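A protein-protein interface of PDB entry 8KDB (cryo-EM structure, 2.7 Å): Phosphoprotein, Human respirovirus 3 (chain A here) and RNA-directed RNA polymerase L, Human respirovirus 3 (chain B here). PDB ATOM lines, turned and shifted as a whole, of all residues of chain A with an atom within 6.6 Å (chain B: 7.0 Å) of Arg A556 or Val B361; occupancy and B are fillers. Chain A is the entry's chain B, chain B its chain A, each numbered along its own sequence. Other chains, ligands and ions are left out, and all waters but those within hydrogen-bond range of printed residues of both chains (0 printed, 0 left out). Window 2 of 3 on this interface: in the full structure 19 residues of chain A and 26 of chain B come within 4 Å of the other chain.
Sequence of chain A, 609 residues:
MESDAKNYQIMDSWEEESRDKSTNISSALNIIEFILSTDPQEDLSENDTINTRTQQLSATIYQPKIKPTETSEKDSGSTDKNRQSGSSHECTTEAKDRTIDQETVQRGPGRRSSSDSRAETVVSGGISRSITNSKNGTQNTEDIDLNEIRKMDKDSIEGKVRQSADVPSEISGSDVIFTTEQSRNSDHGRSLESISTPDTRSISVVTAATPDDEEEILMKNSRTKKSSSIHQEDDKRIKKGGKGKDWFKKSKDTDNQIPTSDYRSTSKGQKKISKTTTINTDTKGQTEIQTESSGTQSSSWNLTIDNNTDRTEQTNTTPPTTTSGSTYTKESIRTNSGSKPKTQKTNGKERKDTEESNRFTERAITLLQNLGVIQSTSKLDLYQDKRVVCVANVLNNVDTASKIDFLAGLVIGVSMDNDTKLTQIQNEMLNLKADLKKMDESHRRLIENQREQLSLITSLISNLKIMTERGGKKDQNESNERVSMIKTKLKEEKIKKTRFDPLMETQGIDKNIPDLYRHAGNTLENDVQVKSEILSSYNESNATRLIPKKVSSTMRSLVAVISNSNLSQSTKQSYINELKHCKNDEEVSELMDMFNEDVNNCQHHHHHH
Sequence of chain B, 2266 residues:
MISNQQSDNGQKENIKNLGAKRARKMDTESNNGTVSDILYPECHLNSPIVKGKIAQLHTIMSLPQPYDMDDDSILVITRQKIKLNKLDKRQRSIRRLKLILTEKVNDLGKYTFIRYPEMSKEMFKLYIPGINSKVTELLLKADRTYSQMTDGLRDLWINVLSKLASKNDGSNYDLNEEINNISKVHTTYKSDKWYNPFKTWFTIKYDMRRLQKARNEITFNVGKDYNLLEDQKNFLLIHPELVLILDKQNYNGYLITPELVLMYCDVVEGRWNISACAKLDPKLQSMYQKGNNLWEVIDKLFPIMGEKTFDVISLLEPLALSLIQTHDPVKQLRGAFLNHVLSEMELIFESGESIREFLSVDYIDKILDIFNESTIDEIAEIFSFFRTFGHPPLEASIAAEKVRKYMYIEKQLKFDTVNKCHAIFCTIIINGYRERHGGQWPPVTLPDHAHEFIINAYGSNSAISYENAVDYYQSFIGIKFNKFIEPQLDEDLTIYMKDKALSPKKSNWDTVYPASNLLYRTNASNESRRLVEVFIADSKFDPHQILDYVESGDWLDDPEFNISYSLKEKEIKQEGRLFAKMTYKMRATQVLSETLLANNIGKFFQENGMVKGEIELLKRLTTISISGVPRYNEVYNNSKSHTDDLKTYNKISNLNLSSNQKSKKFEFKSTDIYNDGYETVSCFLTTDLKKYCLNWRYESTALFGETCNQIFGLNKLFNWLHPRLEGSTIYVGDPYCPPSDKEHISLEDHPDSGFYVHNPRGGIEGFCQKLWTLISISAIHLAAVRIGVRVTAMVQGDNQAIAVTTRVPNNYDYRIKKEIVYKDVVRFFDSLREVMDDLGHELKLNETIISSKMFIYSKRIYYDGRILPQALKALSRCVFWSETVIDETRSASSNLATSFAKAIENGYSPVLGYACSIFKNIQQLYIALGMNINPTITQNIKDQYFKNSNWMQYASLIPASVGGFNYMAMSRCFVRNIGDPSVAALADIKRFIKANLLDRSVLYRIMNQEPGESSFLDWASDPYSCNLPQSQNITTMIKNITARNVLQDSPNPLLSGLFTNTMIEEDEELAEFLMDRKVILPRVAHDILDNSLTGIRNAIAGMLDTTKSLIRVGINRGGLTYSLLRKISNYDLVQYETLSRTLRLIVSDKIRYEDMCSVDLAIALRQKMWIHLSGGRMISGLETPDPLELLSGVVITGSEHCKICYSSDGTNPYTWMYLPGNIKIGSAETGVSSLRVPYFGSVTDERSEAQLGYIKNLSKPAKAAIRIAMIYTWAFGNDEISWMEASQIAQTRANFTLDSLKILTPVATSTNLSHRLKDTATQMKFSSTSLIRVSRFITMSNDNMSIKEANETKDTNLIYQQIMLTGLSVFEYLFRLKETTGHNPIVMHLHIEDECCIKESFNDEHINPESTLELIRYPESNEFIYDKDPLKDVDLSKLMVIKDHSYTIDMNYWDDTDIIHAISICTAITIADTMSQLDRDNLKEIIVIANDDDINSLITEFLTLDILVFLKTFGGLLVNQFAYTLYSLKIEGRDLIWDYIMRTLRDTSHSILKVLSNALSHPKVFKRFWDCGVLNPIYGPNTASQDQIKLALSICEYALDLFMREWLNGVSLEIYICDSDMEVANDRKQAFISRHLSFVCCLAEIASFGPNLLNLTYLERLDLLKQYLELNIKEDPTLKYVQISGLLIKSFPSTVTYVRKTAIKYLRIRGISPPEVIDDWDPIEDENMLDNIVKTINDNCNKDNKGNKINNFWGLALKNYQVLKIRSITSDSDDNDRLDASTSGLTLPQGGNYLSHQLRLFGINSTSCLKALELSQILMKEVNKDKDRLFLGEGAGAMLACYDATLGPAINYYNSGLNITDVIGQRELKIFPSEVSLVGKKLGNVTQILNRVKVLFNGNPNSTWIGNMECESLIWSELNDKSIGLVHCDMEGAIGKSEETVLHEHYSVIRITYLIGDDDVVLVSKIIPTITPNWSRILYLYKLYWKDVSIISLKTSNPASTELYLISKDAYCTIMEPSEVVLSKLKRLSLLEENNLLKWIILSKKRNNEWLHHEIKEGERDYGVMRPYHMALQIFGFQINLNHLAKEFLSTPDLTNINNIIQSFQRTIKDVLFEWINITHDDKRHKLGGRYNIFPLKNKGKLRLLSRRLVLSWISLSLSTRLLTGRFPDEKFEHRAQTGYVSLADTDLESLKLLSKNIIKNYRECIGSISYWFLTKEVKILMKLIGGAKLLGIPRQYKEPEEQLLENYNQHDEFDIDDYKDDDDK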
ATOM      1  N   VAL A 551      23.391 -32.803   6.519  1.00  0.00           N
ATOM      2  CA  VAL A 551      23.667 -31.714   5.591  1.00  0.00           C
ATOM      3  C   VAL A 551      22.641 -30.605   5.796  1.00  0.00           C
ATOM      4  O   VAL A 551      21.505 -30.845   6.225  1.00  0.00           O
ATOM      5  CB  VAL A 551      23.676 -32.216   4.136  1.00  0.00           C
ATOM      6  CG1 VAL A 551      24.672 -33.353   3.976  1.00  0.00           C
ATOM      7  CG2 VAL A 551      22.292 -32.660   3.711  1.00  0.00           C
ATOM      8  N   SER A 552      23.050 -29.370   5.491  1.00  0.00           N
ATOM      9  CA  SER A 552      22.223 -28.210   5.813  1.00  0.00           C
ATOM     10  C   SER A 552      20.888 -28.249   5.080  1.00  0.00           C
ATOM     11  O   SER A 552      19.847 -27.905   5.653  1.00  0.00           O
ATOM     12  CB  SER A 552      22.977 -26.923   5.478  1.00  0.00           C
ATOM     13  OG  SER A 552      23.197 -26.814   4.083  1.00  0.00           O
ATOM     14  N   SER A 553      20.899 -28.662   3.810  1.00  0.00           N
ATOM     15  CA  SER A 553      19.664 -28.702   3.035  1.00  0.00           C
ATOM     16  C   SER A 553      18.648 -29.660   3.645  1.00  0.00           C
ATOM     17  O   SER A 553      17.444 -29.381   3.624  1.00  0.00           O
ATOM     18  CB  SER A 553      19.967 -29.092   1.589  1.00  0.00           C
ATOM     19  OG  SER A 553      18.780 -29.169   0.824  1.00  0.00           O
ATOM     20  N   THR A 554      19.107 -30.787   4.186  1.00  0.00           N
ATOM     21  CA  THR A 554      18.215 -31.712   4.874  1.00  0.00           C
ATOM     22  C   THR A 554      17.823 -31.221   6.261  1.00  0.00           C
ATOM     23  O   THR A 554      16.683 -31.439   6.686  1.00  0.00           O
ATOM     24  CB  THR A 554      18.864 -33.095   4.982  1.00  0.00           C
ATOM     25  OG1 THR A 554      19.247 -33.545   3.677  1.00  0.00           O
ATOM     26  CG2 THR A 554      17.897 -34.101   5.584  1.00  0.00           C
ATOM     27  N   MET A 555      18.735 -30.556   6.975  1.00  0.00           N
ATOM     28  CA  MET A 555      18.401 -30.045   8.302  1.00  0.00           C
ATOM     29  C   MET A 555      17.310 -28.983   8.231  1.00  0.00           C
ATOM     30  O   MET A 555      16.375 -28.986   9.044  1.00  0.00           O
ATOM     31  CB  MET A 555      19.652 -29.484   8.978  1.00  0.00           C
ATOM     32  CG  MET A 555      20.701 -30.532   9.311  1.00  0.00           C
ATOM     33  SD  MET A 555      20.139 -31.720  10.545  1.00  0.00           S
ATOM     34  CE  MET A 555      20.660 -30.911  12.054  1.00  0.00           C
ATOM     35  N   ARG A 556      17.407 -28.067   7.264  1.00  0.00           N
ATOM     36  CA  ARG A 556      16.366 -27.057   7.105  1.00  0.00           C
ATOM     37  C   ARG A 556      15.031 -27.693   6.735  1.00  0.00           C
ATOM     38  O   ARG A 556      13.977 -27.277   7.230  1.00  0.00           O
ATOM     39  CB  ARG A 556      16.780 -26.030   6.053  1.00  0.00           C
ATOM     40  CG  ARG A 556      18.109 -25.355   6.330  1.00  0.00           C
ATOM     41  CD  ARG A 556      18.630 -24.644   5.094  1.00  0.00           C
ATOM     42  NE  ARG A 556      19.585 -23.596   5.429  1.00  0.00           N
ATOM     43  CZ  ARG A 556      19.251 -22.380   5.839  1.00  0.00           C
ATOM     44  NH1 ARG A 556      17.987 -22.021   5.979  1.00  0.00           N
ATOM     45  NH2 ARG A 556      20.211 -21.503   6.115  1.00  0.00           N
ATOM     46  N   SER A 557      15.057 -28.702   5.861  1.00  0.00           N
ATOM     47  CA  SER A 557      13.826 -29.387   5.483  1.00  0.00           C
ATOM     48  C   SER A 557      13.191 -30.081   6.680  1.00  0.00           C
ATOM     49  O   SER A 557      11.968 -30.045   6.851  1.00  0.00           O
ATOM     50  CB  SER A 557      14.110 -30.393   4.368  1.00  0.00           C
ATOM     51  OG  SER A 557      14.938 -29.822   3.372  1.00  0.00           O
ATOM     52  N   LEU A 558      14.008 -30.722   7.519  1.00  0.00           N
ATOM     53  CA  LEU A 558      13.481 -31.374   8.714  1.00  0.00           C
ATOM     54  C   LEU A 558      12.897 -30.358   9.686  1.00  0.00           C
ATOM     55  O   LEU A 558      11.842 -30.600  10.288  1.00  0.00           O
ATOM     56  CB  LEU A 558      14.578 -32.195   9.389  1.00  0.00           C
ATOM     57  CG  LEU A 558      15.062 -33.422   8.617  1.00  0.00           C
ATOM     58  CD1 LEU A 558      16.236 -34.069   9.325  1.00  0.00           C
ATOM     59  CD2 LEU A 558      13.934 -34.418   8.415  1.00  0.00           C
ATOM     60  N   VAL A 559      13.569 -29.217   9.857  1.00  0.00           N
ATOM     61  CA  VAL A 559      13.049 -28.176  10.741  1.00  0.00           C
ATOM     62  C   VAL A 559      11.712 -27.663  10.226  1.00  0.00           C
ATOM     63  O   VAL A 559      10.768 -27.459  10.998  1.00  0.00           O
ATOM     64  CB  VAL A 559      14.076 -27.039  10.893  1.00  0.00           C
ATOM     65  CG1 VAL A 559      13.409 -25.788  11.438  1.00  0.00           C
ATOM     66  CG2 VAL A 559      15.215 -27.471  11.797  1.00  0.00           C
ATOM     67  N   ALA A 560      11.604 -27.458   8.911  1.00  0.00           N
ATOM     68  CA  ALA A 560      10.347 -26.986   8.336  1.00  0.00           C
ATOM     69  C   ALA A 560       9.246 -28.030   8.467  1.00  0.00           C
ATOM     70  O   ALA A 560       8.080 -27.683   8.689  1.00  0.00           O
ATOM     71  CB  ALA A 560      10.551 -26.598   6.874  1.00  0.00           C
ATOM     72  N   VAL A 561       9.589 -29.312   8.320  1.00  0.00           N
ATOM     73  CA  VAL A 561       8.599 -30.372   8.489  1.00  0.00           C
ATOM     74  C   VAL A 561       8.090 -30.400   9.923  1.00  0.00           C
ATOM     75  O   VAL A 561       6.883 -30.526  10.169  1.00  0.00           O
ATOM     76  CB  VAL A 561       9.193 -31.731   8.072  1.00  0.00           C
ATOM     77  CG1 VAL A 561       8.385 -32.874   8.665  1.00  0.00           C
ATOM     78  CG2 VAL A 561       9.246 -31.846   6.560  1.00  0.00           C
ATOM     79  N   LEU B 338      11.276 -30.331  -0.721  1.00  0.00           N
ATOM     80  CA  LEU B 338      11.869 -29.175  -0.061  1.00  0.00           C
ATOM     81  C   LEU B 338      13.384 -29.282   0.008  1.00  0.00           C
ATOM     82  O   LEU B 338      14.077 -28.265  -0.079  1.00  0.00           O
ATOM     83  CB  LEU B 338      11.284 -29.020   1.342  1.00  0.00           C
ATOM     84  CG  LEU B 338      11.681 -27.763   2.114  1.00  0.00           C
ATOM     85  CD1 LEU B 338      11.347 -26.516   1.318  1.00  0.00           C
ATOM     86  CD2 LEU B 338      10.995 -27.733   3.464  1.00  0.00           C
ATOM     87  N   LEU B 342      15.610 -26.286  -1.503  1.00  0.00           N
ATOM     88  CA  LEU B 342      16.525 -25.530  -0.658  1.00  0.00           C
ATOM     89  C   LEU B 342      17.966 -25.693  -1.122  1.00  0.00           C
ATOM     90  O   LEU B 342      18.764 -24.759  -1.009  1.00  0.00           O
ATOM     91  CB  LEU B 342      16.373 -25.956   0.800  1.00  0.00           C
ATOM     92  CG  LEU B 342      15.027 -25.600   1.433  1.00  0.00           C
ATOM     93  CD1 LEU B 342      14.983 -26.027   2.887  1.00  0.00           C
ATOM     94  CD2 LEU B 342      14.744 -24.115   1.296  1.00  0.00           C
ATOM     95  N   MET B 345      18.332 -23.246  -3.891  1.00  0.00           N
ATOM     96  CA  MET B 345      18.413 -21.882  -3.375  1.00  0.00           C
ATOM     97  C   MET B 345      19.775 -21.599  -2.748  1.00  0.00           C
ATOM     98  O   MET B 345      20.318 -20.501  -2.907  1.00  0.00           O
ATOM     99  CB  MET B 345      17.286 -21.620  -2.379  1.00  0.00           C
ATOM    100  CG  MET B 345      15.904 -21.697  -3.001  1.00  0.00           C
ATOM    101  SD  MET B 345      14.798 -20.392  -2.441  1.00  0.00           S
ATOM    102  CE  MET B 345      14.614 -20.829  -0.717  1.00  0.00           C
ATOM    103  N   GLU B 346      20.345 -22.572  -2.030  1.00  0.00           N
ATOM    104  CA  GLU B 346      21.686 -22.389  -1.481  1.00  0.00           C
ATOM    105  C   GLU B 346      22.717 -22.236  -2.590  1.00  0.00           C
ATOM    106  O   GLU B 346      23.635 -21.412  -2.489  1.00  0.00           O
ATOM    107  CB  GLU B 346      22.056 -23.558  -0.569  1.00  0.00           C
ATOM    108  CG  GLU B 346      21.152 -23.722   0.636  1.00  0.00           C
ATOM    109  CD  GLU B 346      21.733 -24.651   1.680  1.00  0.00           C
ATOM    110  OE1 GLU B 346      22.360 -25.660   1.294  1.00  0.00           O
ATOM    111  OE2 GLU B 346      21.560 -24.376   2.885  1.00  0.00           O
ATOM    112  N   PHE B 349      22.423 -18.719  -3.800  1.00  0.00           N
ATOM    113  CA  PHE B 349      22.914 -17.744  -2.835  1.00  0.00           C
ATOM    114  C   PHE B 349      24.407 -17.860  -2.555  1.00  0.00           C
ATOM    115  O   PHE B 349      24.960 -16.979  -1.888  1.00  0.00           O
ATOM    116  CB  PHE B 349      22.141 -17.868  -1.520  1.00  0.00           C
ATOM    117  CG  PHE B 349      20.852 -17.099  -1.499  1.00  0.00           C
ATOM    118  CD1 PHE B 349      19.701 -17.630  -2.053  1.00  0.00           C
ATOM    119  CD2 PHE B 349      20.792 -15.842  -0.926  1.00  0.00           C
ATOM    120  CE1 PHE B 349      18.517 -16.923  -2.035  1.00  0.00           C
ATOM    121  CE2 PHE B 349      19.612 -15.132  -0.905  1.00  0.00           C
ATOM    122  CZ  PHE B 349      18.472 -15.673  -1.460  1.00  0.00           C
ATOM    123  N   GLU B 350      25.072 -18.915  -3.027  1.00  0.00           N
ATOM    124  CA  GLU B 350      26.511 -19.063  -2.841  1.00  0.00           C
ATOM    125  C   GLU B 350      27.292 -18.850  -4.133  1.00  0.00           C
ATOM    126  O   GLU B 350      28.461 -19.242  -4.217  1.00  0.00           O
ATOM    127  CB  GLU B 350      26.840 -20.439  -2.264  1.00  0.00           C
ATOM    128  CG  GLU B 350      26.904 -20.500  -0.752  1.00  0.00           C
ATOM    129  CD  GLU B 350      26.477 -21.853  -0.215  1.00  0.00           C
ATOM    130  OE1 GLU B 350      26.707 -22.865  -0.910  1.00  0.00           O
ATOM    131  OE2 GLU B 350      25.915 -21.910   0.897  1.00  0.00           O
ATOM    132  N   LEU B 359      25.257 -10.636   1.348  1.00  0.00           N
ATOM    133  CA  LEU B 359      24.214 -11.601   1.671  1.00  0.00           C
ATOM    134  C   LEU B 359      24.825 -12.847   2.290  1.00  0.00           C
ATOM    135  O   LEU B 359      25.902 -13.286   1.875  1.00  0.00           O
ATOM    136  CB  LEU B 359      23.417 -11.992   0.424  1.00  0.00           C
ATOM    137  CG  LEU B 359      22.123 -11.234   0.151  1.00  0.00           C
ATOM    138  CD1 LEU B 359      21.368 -11.910  -0.974  1.00  0.00           C
ATOM    139  CD2 LEU B 359      21.287 -11.162   1.407  1.00  0.00           C
ATOM    140  N   SER B 360      24.134 -13.412   3.274  1.00  0.00           N
ATOM    141  CA  SER B 360      24.489 -14.710   3.818  1.00  0.00           C
ATOM    142  C   SER B 360      23.517 -15.767   3.298  1.00  0.00           C
ATOM    143  O   SER B 360      22.604 -15.485   2.518  1.00  0.00           O
ATOM    144  CB  SER B 360      24.494 -14.669   5.344  1.00  0.00           C
ATOM    145  OG  SER B 360      23.173 -14.656   5.856  1.00  0.00           O
ATOM    146  N   VAL B 361      23.719 -17.010   3.737  1.00  0.00           N
ATOM    147  CA  VAL B 361      22.809 -18.086   3.370  1.00  0.00           C
ATOM    148  C   VAL B 361      21.517 -18.006   4.176  1.00  0.00           C
ATOM    149  O   VAL B 361      20.467 -18.469   3.714  1.00  0.00           O
ATOM    150  CB  VAL B 361      23.523 -19.441   3.550  1.00  0.00           C
ATOM    151  CG1 VAL B 361      22.551 -20.606   3.448  1.00  0.00           C
ATOM    152  CG2 VAL B 361      24.635 -19.579   2.530  1.00  0.00           C
ATOM    153  N   ASP B 362      21.555 -17.369   5.344  1.00  0.00           N
ATOM    154  CA  ASP B 362      20.418 -17.280   6.258  1.00  0.00           C
ATOM    155  C   ASP B 362      19.270 -16.435   5.722  1.00  0.00           C
ATOM    156  O   ASP B 362      18.282 -16.265   6.446  1.00  0.00           O
ATOM    157  CB  ASP B 362      20.886 -16.727   7.604  1.00  0.00           C
ATOM    158  CG  ASP B 362      22.185 -17.354   8.070  1.00  0.00           C
ATOM    159  OD1 ASP B 362      22.274 -18.599   8.088  1.00  0.00           O
ATOM    160  OD2 ASP B 362      23.119 -16.600   8.418  1.00  0.00           O
ATOM    161  N   TYR B 363      19.343 -15.900   4.503  1.00  0.00           N
ATOM    162  CA  TYR B 363      18.198 -15.221   3.913  1.00  0.00           C
ATOM    163  C   TYR B 363      17.104 -16.206   3.519  1.00  0.00           C
ATOM    164  O   TYR B 363      15.926 -15.826   3.441  1.00  0.00           O
ATOM    165  CB  TYR B 363      18.664 -14.405   2.706  1.00  0.00           C
ATOM    166  CG  TYR B 363      17.806 -13.205   2.386  1.00  0.00           C
ATOM    167  CD1 TYR B 363      16.568 -13.349   1.786  1.00  0.00           C
ATOM    168  CD2 TYR B 363      18.231 -11.926   2.708  1.00  0.00           C
ATOM    169  CE1 TYR B 363      15.788 -12.252   1.499  1.00  0.00           C
ATOM    170  CE2 TYR B 363      17.458 -10.824   2.428  1.00  0.00           C
ATOM    171  CZ  TYR B 363      16.235 -10.991   1.825  1.00  0.00           C
ATOM    172  OH  TYR B 363      15.455  -9.893   1.544  1.00  0.00           O
ATOM    173  N   ILE B 364      17.473 -17.471   3.306  1.00  0.00           N
ATOM    174  CA  ILE B 364      16.491 -18.518   3.063  1.00  0.00           C
ATOM    175  C   ILE B 364      15.554 -18.662   4.252  1.00  0.00           C
ATOM    176  O   ILE B 364      14.361 -18.929   4.079  1.00  0.00           O
ATOM    177  CB  ILE B 364      17.204 -19.842   2.735  1.00  0.00           C
ATOM    178  CG1 ILE B 364      18.042 -19.690   1.466  1.00  0.00           C
ATOM    179  CG2 ILE B 364      16.206 -20.972   2.580  1.00  0.00           C
ATOM    180  CD1 ILE B 364      18.987 -20.840   1.222  1.00  0.00           C
ATOM    181  N   ASP B 365      16.065 -18.495   5.474  1.00  0.00           N
ATOM    182  CA  ASP B 365      15.189 -18.494   6.641  1.00  0.00           C
ATOM    183  C   ASP B 365      14.208 -17.330   6.605  1.00  0.00           C
ATOM    184  O   ASP B 365      13.045 -17.489   6.990  1.00  0.00           O
ATOM    185  CB  ASP B 365      16.013 -18.455   7.926  1.00  0.00           C
ATOM    186  CG  ASP B 365      17.095 -19.513   7.956  1.00  0.00           C
ATOM    187  OD1 ASP B 365      18.185 -19.268   7.401  1.00  0.00           O
ATOM    188  OD2 ASP B 365      16.855 -20.594   8.535  1.00  0.00           O
ATOM    189  N   LYS B 366      14.656 -16.156   6.154  1.00  0.00           N
ATOM    190  CA  LYS B 366      13.747 -15.021   6.031  1.00  0.00           C
ATOM    191  C   LYS B 366      12.659 -15.294   5.002  1.00  0.00           C
ATOM    192  O   LYS B 366      11.521 -14.840   5.161  1.00  0.00           O
ATOM    193  CB  LYS B 366      14.522 -13.758   5.663  1.00  0.00           C
ATOM    194  CG  LYS B 366      15.385 -13.213   6.781  1.00  0.00           C
ATOM    195  CD  LYS B 366      16.151 -11.989   6.323  1.00  0.00           C
ATOM    196  CE  LYS B 366      15.219 -10.810   6.120  1.00  0.00           C
ATOM    197  NZ  LYS B 366      14.655 -10.326   7.409  1.00  0.00           N
ATOM    198  N   LEU B 368      11.559 -18.418   4.273  1.00  0.00           N
ATOM    199  CA  LEU B 368      10.754 -19.543   4.743  1.00  0.00           C
ATOM    200  C   LEU B 368       9.802 -19.139   5.863  1.00  0.00           C
ATOM    201  O   LEU B 368       8.638 -19.551   5.867  1.00  0.00           O
ATOM    202  CB  LEU B 368      11.660 -20.680   5.213  1.00  0.00           C
ATOM    203  CG  LEU B 368      12.301 -21.571   4.151  1.00  0.00           C
ATOM    204  CD1 LEU B 368      13.289 -22.527   4.796  1.00  0.00           C
ATOM    205  CD2 LEU B 368      11.240 -22.339   3.385  1.00  0.00           C
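O of Ser A553 is in hydrogen-bond range of OG of Ser A557.
NH1 of Arg A556 is in salt-bridge range of OD1 of Asp B365 (3.1 Å). OG of Ser A552 sits at hydrogen-bond distance from OE1 of Glu B346, 3.1 Å away. OE2 of Glu B346 lies within salt-bridge range of NE of Arg A556 (3.3 Å).
Among the printed residues, merely in contact across the chains: Arg A556 with Leu B342 (3.6 Å), Arg A556 with Val B361 (3.7 Å), Arg A556 with Ile B364 (3.98 Å), Ser A557 with Leu B338 (3.7 Å), Ser A557 with Leu B342 (3.8 Å) and Ala A560 with Leu B338 (3.6 Å).
Hydrophobic or aromatic side chains of chain A that line the printed part of chain B: Ala A560. Hydrophobic or aromatic side chains of chain B within 4 Å of the printed part of chain A: Leu B338, Leu B342, Val B361 and Ile B364. Along chain B the printed residues that touch a printed residue of chain A span positions 338 to 365.
Ser A553 touches none of the printed residues of chain B. Arg A556 touches five residues of chain B. Of the printed residues of chain B, Ser A557 touches Leu B338 and Leu B342. Of the printed residues of chain B, Ala A560 touches Leu B338. Of chain A, only Arg A556 (3.7 Å) comes within 4 Å of Val B361. Printed residues of chain A within 4 Å of Ile B364: Arg A556. Lys B366 touches none of the printed residues of chain A.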
